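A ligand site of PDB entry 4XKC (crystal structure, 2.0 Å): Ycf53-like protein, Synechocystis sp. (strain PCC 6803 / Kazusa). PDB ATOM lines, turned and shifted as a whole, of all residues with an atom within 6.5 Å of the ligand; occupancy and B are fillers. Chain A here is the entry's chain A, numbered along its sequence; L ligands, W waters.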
ATOM      1  N   ASP A 109      -1.476  -8.647  -6.597  1.00  0.00           N
ATOM      2  CA  ASP A 109      -1.196 -10.087  -6.600  1.00  0.00           C
ATOM      3  C   ASP A 109      -1.924 -10.786  -7.741  1.00  0.00           C
ATOM      4  O   ASP A 109      -1.339 -11.617  -8.449  1.00  0.00           O
ATOM      5  CB  ASP A 109      -1.594 -10.716  -5.259  1.00  0.00           C
ATOM      6  CG  ASP A 109      -1.134 -12.153  -5.121  1.00  0.00           C
ATOM      7  OD1 ASP A 109       0.082 -12.398  -5.293  1.00  0.00           O
ATOM      8  OD2 ASP A 109      -1.976 -13.031  -4.848  1.00  0.00           O
ATOM      9  N   ARG A 113      -0.149 -12.626 -11.108  1.00  0.00           N
ATOM     10  CA  ARG A 113      -0.446 -14.001 -11.481  1.00  0.00           C
ATOM     11  C   ARG A 113      -0.912 -14.088 -12.934  1.00  0.00           C
ATOM     12  O   ARG A 113      -0.473 -14.961 -13.685  1.00  0.00           O
ATOM     13  CB  ARG A 113      -1.490 -14.605 -10.532  1.00  0.00           C
ATOM     14  CG  ARG A 113      -1.860 -16.047 -10.838  1.00  0.00           C
ATOM     15  CD  ARG A 113      -2.435 -16.759  -9.614  1.00  0.00           C
ATOM     16  NE  ARG A 113      -3.543 -16.016  -9.010  1.00  0.00           N
ATOM     17  CZ  ARG A 113      -3.451 -15.313  -7.880  1.00  0.00           C
ATOM     18  NH1 ARG A 113      -2.297 -15.252  -7.233  1.00  0.00           N
ATOM     19  NH2 ARG A 113      -4.512 -14.676  -7.405  1.00  0.00           N
ATOM     20  N   GLN A 128      -4.433 -21.226 -17.406  1.00  0.00           N
ATOM     21  CA  GLN A 128      -4.381 -20.335 -16.243  1.00  0.00           C
ATOM     22  C   GLN A 128      -3.497 -20.823 -15.100  1.00  0.00           C
ATOM     23  O   GLN A 128      -3.724 -20.486 -13.945  1.00  0.00           O
ATOM     24  CB  GLN A 128      -5.787 -19.960 -15.752  1.00  0.00           C
ATOM     25  CG  GLN A 128      -6.461 -18.893 -16.581  1.00  0.00           C
ATOM     26  CD  GLN A 128      -5.766 -17.542 -16.479  1.00  0.00           C
ATOM     27  OE1 GLN A 128      -5.612 -16.983 -15.382  1.00  0.00           O
ATOM     28  NE2 GLN A 128      -5.333 -17.007 -17.616  1.00  0.00           N
ATOM     29  N   TRP A 129      -2.496 -21.636 -15.429  1.00  0.00           N
ATOM     30  CA  TRP A 129      -1.409 -21.937 -14.500  1.00  0.00           C
ATOM     31  C   TRP A 129      -0.142 -22.290 -15.260  1.00  0.00           C
ATOM     32  O   TRP A 129      -0.185 -22.526 -16.479  1.00  0.00           O
ATOM     33  CB  TRP A 129      -1.797 -23.028 -13.502  1.00  0.00           C
ATOM     34  CG  TRP A 129      -2.479 -24.222 -14.087  1.00  0.00           C
ATOM     35  CD1 TRP A 129      -3.822 -24.348 -14.332  1.00  0.00           C
ATOM     36  CD2 TRP A 129      -1.877 -25.452 -14.478  1.00  0.00           C
ATOM     37  NE1 TRP A 129      -4.077 -25.593 -14.873  1.00  0.00           N
ATOM     38  CE2 TRP A 129      -2.908 -26.288 -14.967  1.00  0.00           C
ATOM     39  CE3 TRP A 129      -0.566 -25.939 -14.467  1.00  0.00           C
ATOM     40  CZ2 TRP A 129      -2.660 -27.576 -15.432  1.00  0.00           C
ATOM     41  CZ3 TRP A 129      -0.329 -27.221 -14.926  1.00  0.00           C
ATOM     42  CH2 TRP A 129      -1.369 -28.020 -15.413  1.00  0.00           C
ATOM     43  N   TRP A 183       3.000 -18.432   4.756  1.00  0.00           N
ATOM     44  CA  TRP A 183       2.170 -19.276   3.901  1.00  0.00           C
ATOM     45  C   TRP A 183       1.749 -20.547   4.627  1.00  0.00           C
ATOM     46  O   TRP A 183       0.881 -21.289   4.153  1.00  0.00           O
ATOM     47  CB  TRP A 183       2.870 -19.596   2.580  1.00  0.00           C
ATOM     48  CG  TRP A 183       3.097 -18.376   1.728  1.00  0.00           C
ATOM     49  CD1 TRP A 183       2.793 -17.092   2.035  1.00  0.00           C
ATOM     50  CD2 TRP A 183       3.695 -18.350   0.417  1.00  0.00           C
ATOM     51  NE1 TRP A 183       3.158 -16.250   1.008  1.00  0.00           N
ATOM     52  CE2 TRP A 183       3.713 -17.007   0.004  1.00  0.00           C
ATOM     53  CE3 TRP A 183       4.208 -19.327  -0.435  1.00  0.00           C
ATOM     54  CZ2 TRP A 183       4.229 -16.622  -1.231  1.00  0.00           C
ATOM     55  CZ3 TRP A 183       4.712 -18.945  -1.658  1.00  0.00           C
ATOM     56  CH2 TRP A 183       4.725 -17.596  -2.041  1.00  0.00           C
ATOM     57  N   TRP A 189      -1.813 -24.892   6.138  1.00  0.00           N
ATOM     58  CA  TRP A 189      -1.541 -23.926   5.082  1.00  0.00           C
ATOM     59  C   TRP A 189      -2.440 -22.705   5.236  1.00  0.00           C
ATOM     60  O   TRP A 189      -3.608 -22.830   5.605  1.00  0.00           O
ATOM     61  CB  TRP A 189      -1.763 -24.548   3.706  1.00  0.00           C
ATOM     62  CG  TRP A 189      -0.706 -25.533   3.314  1.00  0.00           C
ATOM     63  CD1 TRP A 189      -0.704 -26.872   3.540  1.00  0.00           C
ATOM     64  CD2 TRP A 189       0.511 -25.237   2.612  1.00  0.00           C
ATOM     65  NE1 TRP A 189       0.437 -27.439   3.022  1.00  0.00           N
ATOM     66  CE2 TRP A 189       1.198 -26.459   2.451  1.00  0.00           C
ATOM     67  CE3 TRP A 189       1.076 -24.070   2.099  1.00  0.00           C
ATOM     68  CZ2 TRP A 189       2.426 -26.541   1.804  1.00  0.00           C
ATOM     69  CZ3 TRP A 189       2.301 -24.155   1.466  1.00  0.00           C
ATOM     70  CH2 TRP A 189       2.966 -25.380   1.316  1.00  0.00           C
ATOM     71  N   THR A 190      -1.891 -21.529   4.952  1.00  0.00           N
ATOM     72  CA  THR A 190      -2.676 -20.314   4.961  1.00  0.00           C
ATOM     73  C   THR A 190      -3.725 -20.404   3.851  1.00  0.00           C
ATOM     74  O   THR A 190      -3.409 -20.744   2.711  1.00  0.00           O
ATOM     75  CB  THR A 190      -1.781 -19.071   4.745  1.00  0.00           C
ATOM     76  OG1 THR A 190      -0.790 -19.025   5.767  1.00  0.00           O
ATOM     77  CG2 THR A 190      -2.611 -17.807   4.788  1.00  0.00           C
ATOM     78  N   TRP A 192      -6.289 -19.315   1.052  1.00  0.00           N
ATOM     79  CA  TRP A 192      -6.536 -18.239   0.090  1.00  0.00           C
ATOM     80  C   TRP A 192      -8.041 -18.049  -0.088  1.00  0.00           C
ATOM     81  O   TRP A 192      -8.784 -19.021  -0.192  1.00  0.00           O
ATOM     82  CB  TRP A 192      -5.883 -18.577  -1.250  1.00  0.00           C
ATOM     83  CG  TRP A 192      -6.049 -17.514  -2.275  1.00  0.00           C
ATOM     84  CD1 TRP A 192      -5.254 -16.417  -2.464  1.00  0.00           C
ATOM     85  CD2 TRP A 192      -7.081 -17.421  -3.270  1.00  0.00           C
ATOM     86  NE1 TRP A 192      -5.731 -15.652  -3.505  1.00  0.00           N
ATOM     87  CE2 TRP A 192      -6.854 -16.251  -4.009  1.00  0.00           C
ATOM     88  CE3 TRP A 192      -8.180 -18.228  -3.585  1.00  0.00           C
ATOM     89  CZ2 TRP A 192      -7.684 -15.858  -5.063  1.00  0.00           C
ATOM     90  CZ3 TRP A 192      -9.001 -17.834  -4.637  1.00  0.00           C
ATOM     91  CH2 TRP A 192      -8.746 -16.669  -5.358  1.00  0.00           C
ATOM     92  N   PHE A 196      -4.633 -14.668   4.050  1.00  0.00           N
ATOM     93  CA  PHE A 196      -3.436 -13.884   3.755  1.00  0.00           C
ATOM     94  C   PHE A 196      -3.574 -12.428   4.193  1.00  0.00           C
ATOM     95  O   PHE A 196      -4.677 -11.916   4.349  1.00  0.00           O
ATOM     96  CB  PHE A 196      -3.059 -13.986   2.279  1.00  0.00           C
ATOM     97  CG  PHE A 196      -2.618 -15.351   1.864  1.00  0.00           C
ATOM     98  CD1 PHE A 196      -1.305 -15.761   2.065  1.00  0.00           C
ATOM     99  CD2 PHE A 196      -3.517 -16.238   1.297  1.00  0.00           C
ATOM    100  CE1 PHE A 196      -0.900 -17.035   1.696  1.00  0.00           C
ATOM    101  CE2 PHE A 196      -3.110 -17.504   0.923  1.00  0.00           C
ATOM    102  CZ  PHE A 196      -1.806 -17.905   1.117  1.00  0.00           C
ATOM    103  N   TRP A 198      -3.024  -8.673   3.271  1.00  0.00           N
ATOM    104  CA  TRP A 198      -2.847  -7.838   2.092  1.00  0.00           C
ATOM    105  C   TRP A 198      -2.398  -6.411   2.408  1.00  0.00           C
ATOM    106  O   TRP A 198      -2.867  -5.453   1.793  1.00  0.00           O
ATOM    107  CB  TRP A 198      -4.144  -7.801   1.282  1.00  0.00           C
ATOM    108  CG  TRP A 198      -4.679  -9.158   0.947  1.00  0.00           C
ATOM    109  CD1 TRP A 198      -5.762  -9.767   1.505  1.00  0.00           C
ATOM    110  CD2 TRP A 198      -4.155 -10.069  -0.027  1.00  0.00           C
ATOM    111  NE1 TRP A 198      -5.952 -11.012   0.938  1.00  0.00           N
ATOM    112  CE2 TRP A 198      -4.973 -11.218  -0.011  1.00  0.00           C
ATOM    113  CE3 TRP A 198      -3.078 -10.028  -0.913  1.00  0.00           C
ATOM    114  CZ2 TRP A 198      -4.742 -12.307  -0.836  1.00  0.00           C
ATOM    115  CZ3 TRP A 198      -2.856 -11.117  -1.739  1.00  0.00           C
ATOM    116  CH2 TRP A 198      -3.688 -12.236  -1.696  1.00  0.00           C
ATOM    117  N   HIS A 206       5.941 -12.048   2.091  1.00  0.00           N
ATOM    118  CA  HIS A 206       4.569 -12.574   2.074  1.00  0.00           C
ATOM    119  C   HIS A 206       3.955 -12.566   0.671  1.00  0.00           C
ATOM    120  O   HIS A 206       3.216 -13.472   0.304  1.00  0.00           O
ATOM    121  CB  HIS A 206       3.700 -11.749   3.027  1.00  0.00           C
ATOM    122  CG  HIS A 206       2.375 -12.383   3.330  1.00  0.00           C
ATOM    123  ND1 HIS A 206       2.254 -13.633   3.898  1.00  0.00           N
ATOM    124  CD2 HIS A 206       1.108 -11.918   3.173  1.00  0.00           C
ATOM    125  CE1 HIS A 206       0.973 -13.926   4.057  1.00  0.00           C
ATOM    126  NE2 HIS A 206       0.253 -12.894   3.633  1.00  0.00           N
ATOM    127  N   LEU A 209       1.989 -14.099  -4.066  1.00  0.00           N
ATOM    128  CA  LEU A 209       1.691 -15.495  -3.743  1.00  0.00           C
ATOM    129  C   LEU A 209       2.037 -16.441  -4.875  1.00  0.00           C
ATOM    130  O   LEU A 209       1.894 -16.118  -6.059  1.00  0.00           O
ATOM    131  CB  LEU A 209       0.217 -15.651  -3.375  1.00  0.00           C
ATOM    132  CG  LEU A 209      -0.276 -14.833  -2.174  1.00  0.00           C
ATOM    133  CD1 LEU A 209      -1.719 -15.204  -1.848  1.00  0.00           C
ATOM    134  CD2 LEU A 209       0.627 -15.066  -0.971  1.00  0.00           C
ATOM    135  N   LEU A 210       2.498 -17.636  -4.505  1.00  0.00           N
ATOM    136  CA  LEU A 210       2.739 -18.717  -5.452  1.00  0.00           C
ATOM    137  C   LEU A 210       1.983 -19.946  -4.965  1.00  0.00           C
ATOM    138  O   LEU A 210       2.421 -20.624  -4.041  1.00  0.00           O
ATOM    139  CB  LEU A 210       4.242 -19.026  -5.533  1.00  0.00           C
ATOM    140  CG  LEU A 210       5.142 -17.945  -6.121  1.00  0.00           C
ATOM    141  CD1 LEU A 210       6.615 -18.293  -5.899  1.00  0.00           C
ATOM    142  CD2 LEU A 210       4.850 -17.754  -7.601  1.00  0.00           C
ATOM    143  N   ASN A 211       0.841 -20.222  -5.598  1.00  0.00           N
ATOM    144  CA  ASN A 211      -0.017 -21.346  -5.212  1.00  0.00           C
ATOM    145  C   ASN A 211       0.747 -22.660  -5.176  1.00  0.00           C
ATOM    146  O   ASN A 211       1.469 -22.999  -6.129  1.00  0.00           O
ATOM    147  CB  ASN A 211      -1.216 -21.444  -6.150  1.00  0.00           C
ATOM    148  CG  ASN A 211      -2.301 -22.383  -5.639  1.00  0.00           C
ATOM    149  OD1 ASN A 211      -2.331 -22.771  -4.463  1.00  0.00           O
ATOM    150  ND2 ASN A 211      -3.232 -22.746  -6.530  1.00  0.00           N
ATOM    151  N   GLN A 212       0.609 -23.400  -4.085  1.00  0.00           N
ATOM    152  CA  GLN A 212       1.323 -24.652  -3.916  1.00  0.00           C
ATOM    153  C   GLN A 212       0.453 -25.867  -4.220  1.00  0.00           C
ATOM    154  O   GLN A 212       0.826 -27.001  -3.924  1.00  0.00           O
ATOM    155  CB  GLN A 212       1.914 -24.741  -2.515  1.00  0.00           C
ATOM    156  CG  GLN A 212       3.010 -23.728  -2.267  1.00  0.00           C
ATOM    157  CD  GLN A 212       4.150 -23.877  -3.264  1.00  0.00           C
ATOM    158  OE1 GLN A 212       4.751 -24.947  -3.363  1.00  0.00           O
ATOM    159  NE2 GLN A 212       4.436 -22.814  -4.012  1.00  0.00           N
ATOM    160  N   LEU A 213      -0.709 -25.619  -4.821  1.00  0.00           N
ATOM    161  CA  LEU A 213      -1.620 -26.686  -5.221  1.00  0.00           C
ATOM    162  C   LEU A 213      -0.940 -27.710  -6.116  1.00  0.00           C
ATOM    163  O   LEU A 213      -1.241 -28.904  -6.046  1.00  0.00           O
ATOM    164  CB  LEU A 213      -2.843 -26.094  -5.945  1.00  0.00           C
ATOM    165  CG  LEU A 213      -3.829 -27.089  -6.554  1.00  0.00           C
ATOM    166  CD1 LEU A 213      -4.396 -28.009  -5.485  1.00  0.00           C
ATOM    167  CD2 LEU A 213      -4.946 -26.358  -7.277  1.00  0.00           C
ATOM    168  N   ARG A 214      -0.001 -27.255  -6.943  1.00  0.00           N
ATOM    169  CA  ARG A 214       0.699 -28.147  -7.868  1.00  0.00           C
ATOM    170  C   ARG A 214       2.177 -28.324  -7.514  1.00  0.00           C
ATOM    171  O   ARG A 214       3.000 -28.585  -8.393  1.00  0.00           O
ATOM    172  CB  ARG A 214       0.542 -27.645  -9.306  1.00  0.00           C
ATOM    173  CG  ARG A 214      -0.914 -27.548  -9.750  1.00  0.00           C
ATOM    174  CD  ARG A 214      -1.088 -26.599 -10.931  1.00  0.00           C
ATOM    175  NE  ARG A 214      -2.384 -25.919 -10.869  1.00  0.00           N
ATOM    176  CZ  ARG A 214      -2.547 -24.673 -10.437  1.00  0.00           C
ATOM    177  NH1 ARG A 214      -1.507 -23.956 -10.029  1.00  0.00           N
ATOM    178  NH2 ARG A 214      -3.762 -24.138 -10.405  1.00  0.00           N
HETATM  179  C1  LIG L   1       0.381 -19.123  -1.107  1.00  0.00           C
HETATM  180  C2  LIG L   1      -1.053 -26.702  -0.400  1.00  0.00           C
HETATM  181  C3  LIG L   1      -3.048 -17.490  -4.715  1.00  0.00           C
HETATM  182  C4  LIG L   1      -7.761 -26.035  -4.349  1.00  0.00           C
HETATM  183  C5  LIG L   1      -5.444 -18.825  -6.321  1.00  0.00           C
HETATM  184  C6  LIG L   1      -4.920 -19.031  -7.725  1.00  0.00           C
HETATM  185  C7  LIG L   1      -5.171 -20.346  -8.363  1.00  0.00           C
HETATM  186  O1  LIG L   1      -6.337 -20.832  -8.329  1.00  0.00           O
HETATM  187  C8  LIG L   1      -8.230 -23.331  -6.004  1.00  0.00           C
HETATM  188  C9  LIG L   1      -7.881 -23.265  -7.457  1.00  0.00           C
HETATM  189  C10 LIG L   1      -8.868 -23.736  -8.467  1.00  0.00           C
HETATM  190  O2  LIG L   1      -8.560 -23.758  -9.684  1.00  0.00           O
HETATM  191  C11 LIG L   1      -4.656 -19.452  -5.178  1.00  0.00           C
HETATM  192  C12 LIG L   1      -3.622 -18.868  -4.501  1.00  0.00           C
HETATM  193  C13 LIG L   1      -3.235 -19.817  -3.572  1.00  0.00           C
HETATM  194  N1  LIG L   1      -3.929 -21.009  -3.583  1.00  0.00           N
HETATM  195  C14 LIG L   1      -4.816 -20.715  -4.620  1.00  0.00           C
HETATM  196  C15 LIG L   1      -2.105 -19.389  -2.704  1.00  0.00           C
HETATM  197  C16 LIG L   1      -1.558 -20.581  -2.054  1.00  0.00           C
HETATM  198  C17 LIG L   1      -0.397 -20.392  -1.307  1.00  0.00           C
HETATM  199  C18 LIG L   1      -0.110 -21.643  -0.811  1.00  0.00           C
HETATM  200  C19 LIG L   1      -1.113 -22.474  -1.285  1.00  0.00           C
HETATM  201  N2  LIG L   1      -2.020 -21.842  -2.071  1.00  0.00           N
HETATM  202  C20 LIG L   1      -1.029 -23.870  -0.883  1.00  0.00           C
HETATM  203  C21 LIG L   1      -2.201 -24.573  -1.354  1.00  0.00           C
HETATM  204  C22 LIG L   1      -2.142 -25.926  -1.100  1.00  0.00           C
HETATM  205  C23 LIG L   1      -3.302 -26.416  -1.604  1.00  0.00           C
HETATM  206  C24 LIG L   1      -3.954 -25.322  -2.127  1.00  0.00           C
HETATM  207  N3  LIG L   1      -3.307 -24.120  -2.012  1.00  0.00           N
HETATM  208  C25 LIG L   1      -5.245 -25.693  -2.735  1.00  0.00           C
HETATM  209  C26 LIG L   1      -5.728 -24.596  -3.613  1.00  0.00           C
HETATM  210  C27 LIG L   1      -6.894 -24.806  -4.337  1.00  0.00           C
HETATM  211  C28 LIG L   1      -7.089 -23.655  -5.042  1.00  0.00           C
HETATM  212  C29 LIG L   1      -6.016 -22.823  -4.688  1.00  0.00           C
HETATM  213  N4  LIG L   1      -5.160 -23.388  -3.820  1.00  0.00           N
HETATM  214  C30 LIG L   1      -5.928 -21.479  -5.281  1.00  0.00           C
HETATM  215 MG1  LIG L   1      -3.843 -22.460  -2.699  1.00  0.00          MG
HETATM  216  O3  LIG L   1     -10.012 -24.100  -8.102  1.00  0.00           O
HETATM  217  O4  LIG L   1      -4.247 -20.962  -8.930  1.00  0.00           O
HETATM  218  O   HOH W   1     -10.042 -23.173 -11.621  1.00  0.00           O
HETATM  219  O   HOH W   2      -8.681 -19.814  -8.552  1.00  0.00           O
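MG1 of the ligand is bound by OD1 of Asn 211 (2.3 Å).
An oxygen (O4) of the ligand lies within salt-bridge range of the guanidinium group (NH2) of Arg 214.
OD1 of Asn 211 sits close to N of Leu 213, at 3.3 Å.
NE2 of Gln 212 is in hydrogen-bond range of O of Leu 210 (3.0 Å).
The side-chain carboxylate (OD2) of Asp 109 is in salt-bridge range of the guanidinium group (NH1) of Arg 113 (3.3 Å).
O of Trp 183 lies within hydrogen-bond range of N of Thr 190, at 2.9 Å.
NE1 of Trp 183 lies within hydrogen-bond range of O of His 206, 2.9 Å away.
N of Leu 209 sits at hydrogen-bond distance from OD1 of Asp 109.
Arg 113 touches the ligand (NH1 to C3, 3.5 Å).
Trp 183 touches the ligand.
CE2 of Trp 189 touches C2 of the ligand, 3.6 Å away.
CD1 of Trp 192 touches C3 of the ligand (3.3 Å).
Phe 196 touches the ligand (CZ to C1, 3.3 Å).
Leu 209 touches the ligand.
O of Leu 210 touches C1 of the ligand, at 3.9 Å.
Gln 212 touches the ligand (N to C19, 3.4 Å).
CD1 of Leu 213 touches C25 of the ligand (3.7 Å).
Within 4 Å of the ligand: Arg 113, Trp 183, Trp 189, Trp 192, Phe 196, Leu 209, Leu 210, Asn 211, Gln 212, Leu 213 and Arg 214.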
